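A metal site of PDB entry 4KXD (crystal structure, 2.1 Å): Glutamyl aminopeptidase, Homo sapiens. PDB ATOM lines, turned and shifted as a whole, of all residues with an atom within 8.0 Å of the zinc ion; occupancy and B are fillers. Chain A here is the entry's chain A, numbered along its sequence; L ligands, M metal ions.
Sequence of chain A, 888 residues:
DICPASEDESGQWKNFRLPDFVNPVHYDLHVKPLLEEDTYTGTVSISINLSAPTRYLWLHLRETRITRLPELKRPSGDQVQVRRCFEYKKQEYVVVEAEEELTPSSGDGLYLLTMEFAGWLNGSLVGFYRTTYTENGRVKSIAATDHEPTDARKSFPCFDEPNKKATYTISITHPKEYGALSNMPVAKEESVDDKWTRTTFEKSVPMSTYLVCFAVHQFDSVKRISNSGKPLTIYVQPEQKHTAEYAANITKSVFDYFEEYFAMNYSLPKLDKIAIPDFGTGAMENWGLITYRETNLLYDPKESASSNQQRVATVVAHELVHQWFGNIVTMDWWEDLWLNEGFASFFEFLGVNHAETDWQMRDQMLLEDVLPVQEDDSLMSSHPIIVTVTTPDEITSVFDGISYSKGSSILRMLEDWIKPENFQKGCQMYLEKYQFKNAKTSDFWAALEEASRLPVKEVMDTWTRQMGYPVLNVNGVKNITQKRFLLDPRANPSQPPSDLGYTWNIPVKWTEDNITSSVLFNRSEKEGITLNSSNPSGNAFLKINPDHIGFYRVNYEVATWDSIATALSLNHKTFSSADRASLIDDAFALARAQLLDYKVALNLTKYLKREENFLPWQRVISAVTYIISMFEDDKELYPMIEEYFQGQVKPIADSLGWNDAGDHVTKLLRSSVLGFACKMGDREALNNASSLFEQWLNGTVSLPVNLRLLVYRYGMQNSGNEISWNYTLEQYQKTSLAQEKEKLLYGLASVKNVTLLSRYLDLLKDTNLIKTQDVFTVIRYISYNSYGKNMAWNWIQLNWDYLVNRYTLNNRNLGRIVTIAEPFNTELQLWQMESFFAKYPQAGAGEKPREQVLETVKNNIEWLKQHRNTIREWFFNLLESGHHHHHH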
ATOM      1  N   GLU A 148      22.981  -2.279 -29.205  1.00  0.00           N
ATOM      2  CA  GLU A 148      22.509  -3.197 -28.155  1.00  0.00           C
ATOM      3  C   GLU A 148      21.527  -2.531 -27.203  1.00  0.00           C
ATOM      4  O   GLU A 148      21.804  -1.450 -26.671  1.00  0.00           O
ATOM      5  CB  GLU A 148      23.672  -3.845 -27.393  1.00  0.00           C
ATOM      6  CG  GLU A 148      23.327  -5.126 -26.630  1.00  0.00           C
ATOM      7  CD  GLU A 148      24.538  -5.771 -25.955  1.00  0.00           C
ATOM      8  OE1 GLU A 148      25.528  -5.052 -25.683  1.00  0.00           O
ATOM      9  OE2 GLU A 148      24.495  -6.982 -25.681  1.00  0.00           O
ATOM     10  N   ALA A 283      30.369   1.572 -22.941  1.00  0.00           N
ATOM     11  CA  ALA A 283      31.098   1.029 -24.078  1.00  0.00           C
ATOM     12  C   ALA A 283      30.304  -0.106 -24.697  1.00  0.00           C
ATOM     13  O   ALA A 283      29.361  -0.615 -24.088  1.00  0.00           O
ATOM     14  CB  ALA A 283      32.470   0.542 -23.640  1.00  0.00           C
ATOM     15  N   MET A 284      30.680  -0.488 -25.912  1.00  0.00           N
ATOM     16  CA  MET A 284      30.003  -1.518 -26.656  1.00  0.00           C
ATOM     17  C   MET A 284      31.027  -2.394 -27.379  1.00  0.00           C
ATOM     18  O   MET A 284      31.969  -1.885 -27.987  1.00  0.00           O
ATOM     19  CB  MET A 284      29.003  -0.893 -27.630  1.00  0.00           C
ATOM     20  CG  MET A 284      28.141  -1.889 -28.384  1.00  0.00           C
ATOM     21  SD  MET A 284      27.274  -3.053 -27.326  1.00  0.00           S
ATOM     22  CE  MET A 284      26.737  -4.248 -28.545  1.00  0.00           C
ATOM     23  N   GLU A 285      30.844  -3.710 -27.298  1.00  0.00           N
ATOM     24  CA  GLU A 285      31.831  -4.675 -27.734  1.00  0.00           C
ATOM     25  C   GLU A 285      31.740  -5.027 -29.219  1.00  0.00           C
ATOM     26  O   GLU A 285      32.143  -6.132 -29.619  1.00  0.00           O
ATOM     27  CB  GLU A 285      31.676  -5.970 -26.944  1.00  0.00           C
ATOM     28  CG  GLU A 285      30.309  -6.617 -27.102  1.00  0.00           C
ATOM     29  CD  GLU A 285      29.311  -6.194 -26.034  1.00  0.00           C
ATOM     30  OE1 GLU A 285      29.595  -5.247 -25.253  1.00  0.00           O
ATOM     31  OE2 GLU A 285      28.233  -6.816 -25.981  1.00  0.00           O
ATOM     32  N   VAL A 315      37.142  -1.483 -18.088  1.00  0.00           N
ATOM     33  CA  VAL A 315      36.188  -1.400 -19.211  1.00  0.00           C
ATOM     34  C   VAL A 315      36.839  -1.987 -20.463  1.00  0.00           C
ATOM     35  O   VAL A 315      36.222  -2.777 -21.177  1.00  0.00           O
ATOM     36  CB  VAL A 315      35.633   0.011 -19.460  1.00  0.00           C
ATOM     37  CG1 VAL A 315      34.651   0.009 -20.618  1.00  0.00           C
ATOM     38  CG2 VAL A 315      34.916   0.528 -18.228  1.00  0.00           C
ATOM     39  N   HIS A 318      36.861  -5.637 -19.922  1.00  0.00           N
ATOM     40  CA  HIS A 318      35.452  -6.026 -20.051  1.00  0.00           C
ATOM     41  C   HIS A 318      35.093  -6.243 -21.507  1.00  0.00           C
ATOM     42  O   HIS A 318      34.579  -7.302 -21.871  1.00  0.00           O
ATOM     43  CB  HIS A 318      34.544  -4.966 -19.438  1.00  0.00           C
ATOM     44  CG  HIS A 318      33.094  -5.346 -19.385  1.00  0.00           C
ATOM     45  ND1 HIS A 318      32.512  -5.894 -18.253  1.00  0.00           N
ATOM     46  CD2 HIS A 318      32.118  -5.272 -20.312  1.00  0.00           C
ATOM     47  CE1 HIS A 318      31.232  -6.127 -18.495  1.00  0.00           C
ATOM     48  NE2 HIS A 318      30.971  -5.759 -19.736  1.00  0.00           N
ATOM     49  N   GLU A 319      35.366  -5.236 -22.335  1.00  0.00           N
ATOM     50  CA  GLU A 319      35.002  -5.270 -23.749  1.00  0.00           C
ATOM     51  C   GLU A 319      35.778  -6.343 -24.490  1.00  0.00           C
ATOM     52  O   GLU A 319      35.259  -6.952 -25.404  1.00  0.00           O
ATOM     53  CB  GLU A 319      35.207  -3.895 -24.404  1.00  0.00           C
ATOM     54  CG  GLU A 319      34.385  -2.762 -23.824  1.00  0.00           C
ATOM     55  CD  GLU A 319      32.942  -3.118 -23.601  1.00  0.00           C
ATOM     56  OE1 GLU A 319      32.314  -3.701 -24.504  1.00  0.00           O
ATOM     57  OE2 GLU A 319      32.409  -2.832 -22.517  1.00  0.00           O
ATOM     58  N   VAL A 321      36.737  -9.236 -23.120  1.00  0.00           N
ATOM     59  CA  VAL A 321      36.129 -10.534 -22.777  1.00  0.00           C
ATOM     60  C   VAL A 321      35.038 -10.871 -23.783  1.00  0.00           C
ATOM     61  O   VAL A 321      34.938 -12.007 -24.255  1.00  0.00           O
ATOM     62  CB  VAL A 321      35.513 -10.574 -21.355  1.00  0.00           C
ATOM     63  CG1 VAL A 321      34.987 -11.962 -21.052  1.00  0.00           C
ATOM     64  CG2 VAL A 321      36.523 -10.156 -20.311  1.00  0.00           C
ATOM     65  N   HIS A 322      34.232  -9.869 -24.117  1.00  0.00           N
ATOM     66  CA  HIS A 322      33.129 -10.045 -25.054  1.00  0.00           C
ATOM     67  C   HIS A 322      33.552 -10.555 -26.422  1.00  0.00           C
ATOM     68  O   HIS A 322      32.751 -11.197 -27.112  1.00  0.00           O
ATOM     69  CB  HIS A 322      32.345  -8.743 -25.228  1.00  0.00           C
ATOM     70  CG  HIS A 322      31.382  -8.456 -24.120  1.00  0.00           C
ATOM     71  ND1 HIS A 322      30.399  -9.350 -23.735  1.00  0.00           N
ATOM     72  CD2 HIS A 322      31.211  -7.360 -23.350  1.00  0.00           C
ATOM     73  CE1 HIS A 322      29.686  -8.808 -22.758  1.00  0.00           C
ATOM     74  NE2 HIS A 322      30.154  -7.606 -22.506  1.00  0.00           N
ATOM     75  N   PHE A 325      33.278 -14.153 -25.001  1.00  0.00           N
ATOM     76  CA  PHE A 325      31.965 -14.370 -24.398  1.00  0.00           C
ATOM     77  C   PHE A 325      31.000 -13.260 -24.760  1.00  0.00           C
ATOM     78  O   PHE A 325      31.003 -12.175 -24.175  1.00  0.00           O
ATOM     79  CB  PHE A 325      32.077 -14.540 -22.890  1.00  0.00           C
ATOM     80  CG  PHE A 325      32.650 -15.864 -22.480  1.00  0.00           C
ATOM     81  CD1 PHE A 325      31.834 -16.984 -22.379  1.00  0.00           C
ATOM     82  CD2 PHE A 325      34.007 -15.993 -22.219  1.00  0.00           C
ATOM     83  CE1 PHE A 325      32.368 -18.214 -22.004  1.00  0.00           C
ATOM     84  CE2 PHE A 325      34.546 -17.223 -21.858  1.00  0.00           C
ATOM     85  CZ  PHE A 325      33.724 -18.333 -21.744  1.00  0.00           C
ATOM     86  N   LEU A 337      21.131 -13.168 -20.983  1.00  0.00           N
ATOM     87  CA  LEU A 337      22.094 -12.058 -21.104  1.00  0.00           C
ATOM     88  C   LEU A 337      23.296 -12.173 -20.175  1.00  0.00           C
ATOM     89  O   LEU A 337      24.406 -11.776 -20.540  1.00  0.00           O
ATOM     90  CB  LEU A 337      21.407 -10.713 -20.852  1.00  0.00           C
ATOM     91  CG  LEU A 337      22.249  -9.437 -20.923  1.00  0.00           C
ATOM     92  CD1 LEU A 337      22.844  -9.218 -22.318  1.00  0.00           C
ATOM     93  CD2 LEU A 337      21.416  -8.239 -20.497  1.00  0.00           C
ATOM     94  N   ASN A 340      26.618 -13.268 -21.368  1.00  0.00           N
ATOM     95  CA  ASN A 340      27.456 -12.216 -21.933  1.00  0.00           C
ATOM     96  C   ASN A 340      28.046 -11.370 -20.818  1.00  0.00           C
ATOM     97  O   ASN A 340      29.264 -11.309 -20.643  1.00  0.00           O
ATOM     98  CB  ASN A 340      26.638 -11.322 -22.866  1.00  0.00           C
ATOM     99  CG  ASN A 340      26.489 -11.892 -24.274  1.00  0.00           C
ATOM    100  OD1 ASN A 340      26.351 -11.137 -25.230  1.00  0.00           O
ATOM    101  ND2 ASN A 340      26.521 -13.214 -24.406  1.00  0.00           N
ATOM    102  N   GLU A 341      27.167 -10.726 -20.061  1.00  0.00           N
ATOM    103  CA  GLU A 341      27.546  -9.662 -19.157  1.00  0.00           C
ATOM    104  C   GLU A 341      28.216 -10.124 -17.867  1.00  0.00           C
ATOM    105  O   GLU A 341      29.156  -9.477 -17.381  1.00  0.00           O
ATOM    106  CB  GLU A 341      26.353  -8.759 -18.855  1.00  0.00           C
ATOM    107  CG  GLU A 341      25.725  -8.150 -20.110  1.00  0.00           C
ATOM    108  CD  GLU A 341      26.679  -7.300 -20.916  1.00  0.00           C
ATOM    109  OE1 GLU A 341      27.807  -7.043 -20.467  1.00  0.00           O
ATOM    110  OE2 GLU A 341      26.305  -6.874 -22.026  1.00  0.00           O
ATOM    111  N   GLY A 342      27.707 -11.231 -17.321  1.00  0.00           N
ATOM    112  CA  GLY A 342      28.270 -11.810 -16.106  1.00  0.00           C
ATOM    113  C   GLY A 342      29.676 -12.318 -16.338  1.00  0.00           C
ATOM    114  O   GLY A 342      30.541 -12.158 -15.492  1.00  0.00           O
ATOM    115  N   PHE A 343      29.882 -12.924 -17.503  1.00  0.00           N
ATOM    116  CA  PHE A 343      31.195 -13.429 -17.892  1.00  0.00           C
ATOM    117  C   PHE A 343      32.196 -12.306 -18.096  1.00  0.00           C
ATOM    118  O   PHE A 343      33.321 -12.370 -17.597  1.00  0.00           O
ATOM    119  CB  PHE A 343      31.104 -14.310 -19.135  1.00  0.00           C
ATOM    120  CG  PHE A 343      30.533 -15.664 -18.847  1.00  0.00           C
ATOM    121  CD1 PHE A 343      29.200 -15.819 -18.470  1.00  0.00           C
ATOM    122  CD2 PHE A 343      31.320 -16.800 -18.941  1.00  0.00           C
ATOM    123  CE1 PHE A 343      28.669 -17.067 -18.187  1.00  0.00           C
ATOM    124  CE2 PHE A 343      30.808 -18.055 -18.666  1.00  0.00           C
ATOM    125  CZ  PHE A 343      29.471 -18.180 -18.290  1.00  0.00           C
ATOM    126  N   ALA A 344      31.781 -11.260 -18.824  1.00  0.00           N
ATOM    127  CA  ALA A 344      32.604 -10.070 -18.989  1.00  0.00           C
ATOM    128  C   ALA A 344      32.916  -9.418 -17.638  1.00  0.00           C
ATOM    129  O   ALA A 344      34.061  -9.061 -17.369  1.00  0.00           O
ATOM    130  CB  ALA A 344      31.946  -9.093 -19.934  1.00  0.00           C
ATOM    131  N   SER A 345      31.894  -9.306 -16.785  1.00  0.00           N
ATOM    132  CA  SER A 345      32.063  -8.725 -15.452  1.00  0.00           C
ATOM    133  C   SER A 345      32.972  -9.577 -14.551  1.00  0.00           C
ATOM    134  O   SER A 345      33.610  -9.042 -13.638  1.00  0.00           O
ATOM    135  CB  SER A 345      30.708  -8.511 -14.747  1.00  0.00           C
ATOM    136  OG  SER A 345      29.857  -7.668 -15.498  1.00  0.00           O
ATOM    137  N   GLU A 348      36.838  -9.626 -16.498  1.00  0.00           N
ATOM    138  CA  GLU A 348      37.451  -8.300 -16.528  1.00  0.00           C
ATOM    139  C   GLU A 348      38.493  -8.138 -15.410  1.00  0.00           C
ATOM    140  O   GLU A 348      39.522  -7.506 -15.617  1.00  0.00           O
ATOM    141  CB  GLU A 348      36.402  -7.181 -16.482  1.00  0.00           C
ATOM    142  CG  GLU A 348      35.710  -7.002 -15.144  1.00  0.00           C
ATOM    143  CD  GLU A 348      34.678  -5.892 -15.138  1.00  0.00           C
ATOM    144  OE1 GLU A 348      34.427  -5.325 -14.059  1.00  0.00           O
ATOM    145  OE2 GLU A 348      34.098  -5.594 -16.202  1.00  0.00           O
ATOM    146  N   PHE A 399      19.811  -5.180 -18.458  1.00  0.00           N
ATOM    147  CA  PHE A 399      21.207  -4.764 -18.424  1.00  0.00           C
ATOM    148  C   PHE A 399      21.414  -4.066 -17.074  1.00  0.00           C
ATOM    149  O   PHE A 399      21.416  -2.842 -16.993  1.00  0.00           O
ATOM    150  CB  PHE A 399      21.514  -3.821 -19.590  1.00  0.00           C
ATOM    151  CG  PHE A 399      21.611  -4.527 -20.930  1.00  0.00           C
ATOM    152  CD1 PHE A 399      20.469  -4.814 -21.665  1.00  0.00           C
ATOM    153  CD2 PHE A 399      22.848  -4.894 -21.450  1.00  0.00           C
ATOM    154  CE1 PHE A 399      20.557  -5.468 -22.885  1.00  0.00           C
ATOM    155  CE2 PHE A 399      22.944  -5.537 -22.674  1.00  0.00           C
ATOM    156  CZ  PHE A 399      21.802  -5.833 -23.387  1.00  0.00           C
ATOM    157  N   TYR A 404      25.079  -8.284 -14.519  1.00  0.00           N
ATOM    158  CA  TYR A 404      26.503  -7.963 -14.402  1.00  0.00           C
ATOM    159  C   TYR A 404      27.114  -8.442 -13.074  1.00  0.00           C
ATOM    160  O   TYR A 404      28.009  -9.287 -13.065  1.00  0.00           O
ATOM    161  CB  TYR A 404      26.732  -6.450 -14.543  1.00  0.00           C
ATOM    162  CG  TYR A 404      26.570  -5.891 -15.953  1.00  0.00           C
ATOM    163  CD1 TYR A 404      25.301  -5.707 -16.520  1.00  0.00           C
ATOM    164  CD2 TYR A 404      27.678  -5.514 -16.699  1.00  0.00           C
ATOM    165  CE1 TYR A 404      25.160  -5.182 -17.794  1.00  0.00           C
ATOM    166  CE2 TYR A 404      27.546  -4.988 -17.977  1.00  0.00           C
ATOM    167  CZ  TYR A 404      26.287  -4.822 -18.525  1.00  0.00           C
ATOM    168  OH  TYR A 404      26.151  -4.306 -19.790  1.00  0.00           O
HETATM  169  N1  LIG L   1      27.675  -4.280 -23.205  1.00  0.00           N
HETATM  170  C1  LIG L   1      27.968  -2.868 -22.840  1.00  0.00           C
HETATM  171  C2  LIG L   1      28.794  -2.732 -21.571  1.00  0.00           C
HETATM  172  O1  LIG L   1      29.933  -2.263 -21.604  1.00  0.00           O
HETATM  173  C3  LIG L   1      26.681  -2.052 -22.698  1.00  0.00           C
HETATM  174  C4  LIG L   1      25.947  -1.802 -23.996  1.00  0.00           C
HETATM  175  C5  LIG L   1      24.559  -1.221 -23.778  1.00  0.00           C
HETATM  176  O2  LIG L   1      23.946  -1.482 -22.733  1.00  0.00           O
HETATM  177  O3  LIG L   1      24.071  -0.482 -24.657  1.00  0.00           O
HETATM  178  O4  LIG L   1      28.358  -3.079 -20.475  1.00  0.00           O
HETATM  179 ZN    ZN M   1      29.313  -6.046 -21.254  1.00  0.00          ZN
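The side-chain hydroxyl of Tyr 404 sits close to the side-chain carboxylate of Glu 341, at 3.4 Å.
The backbone carbonyl oxygen (O) of Glu 341 lies within hydrogen-bond range of the side-chain hydroxyl (OG) of Ser 345 (2.7 Å).
The backbone carbonyl oxygen (O) of Phe 325 is in hydrogen-bond range of a ring nitrogen (ND1) of His 322 (2.9 Å).
A ring nitrogen (ND1) of His 318 is in hydrogen-bond range of the side-chain carboxylate (OE2) of Glu 348 (2.6 Å).
The backbone carbonyl oxygen (O) of Tyr 404 sits close to the side-chain hydroxyl (OG) of Ser 345, at 3.5 Å.
The side-chain carboxylate (OE2) of Glu 341 is in salt-bridge range of a nitrogen (N1) of the ligand (3.2 Å).
The side-chain hydroxyl (OH) of Tyr 404 is in hydrogen-bond range of an oxygen (O4) of the ligand, at 2.6 Å.
A nitrogen (N1) of the ligand is in salt-bridge range of the side-chain carboxylate of Glu 285 (3.0 Å).
An oxygen (O1) of the ligand lies close to the side-chain carboxylate of Glu 319.
The side-chain carboxylate (OE1) of Glu 148 is in salt-bridge range of a nitrogen (N1) of the ligand, 3.4 Å away.
The backbone carbonyl oxygen of Ala 283 lies close to an oxygen (O1) of the ligand, 3.0 Å away.
The zinc ion is bound by OE1 of Glu 341.
NE2 of His 322 is bound to the zinc ion, at 2.2 Å.
The zinc ion is bound by NE2 of His 318.
The zinc ion has three donor atoms within binding distance.
Merely in contact with the zinc ion: Tyr 404 (3.9 Å).
Of the 20 residues printed, 4 come within 4 Å of the zinc ion.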
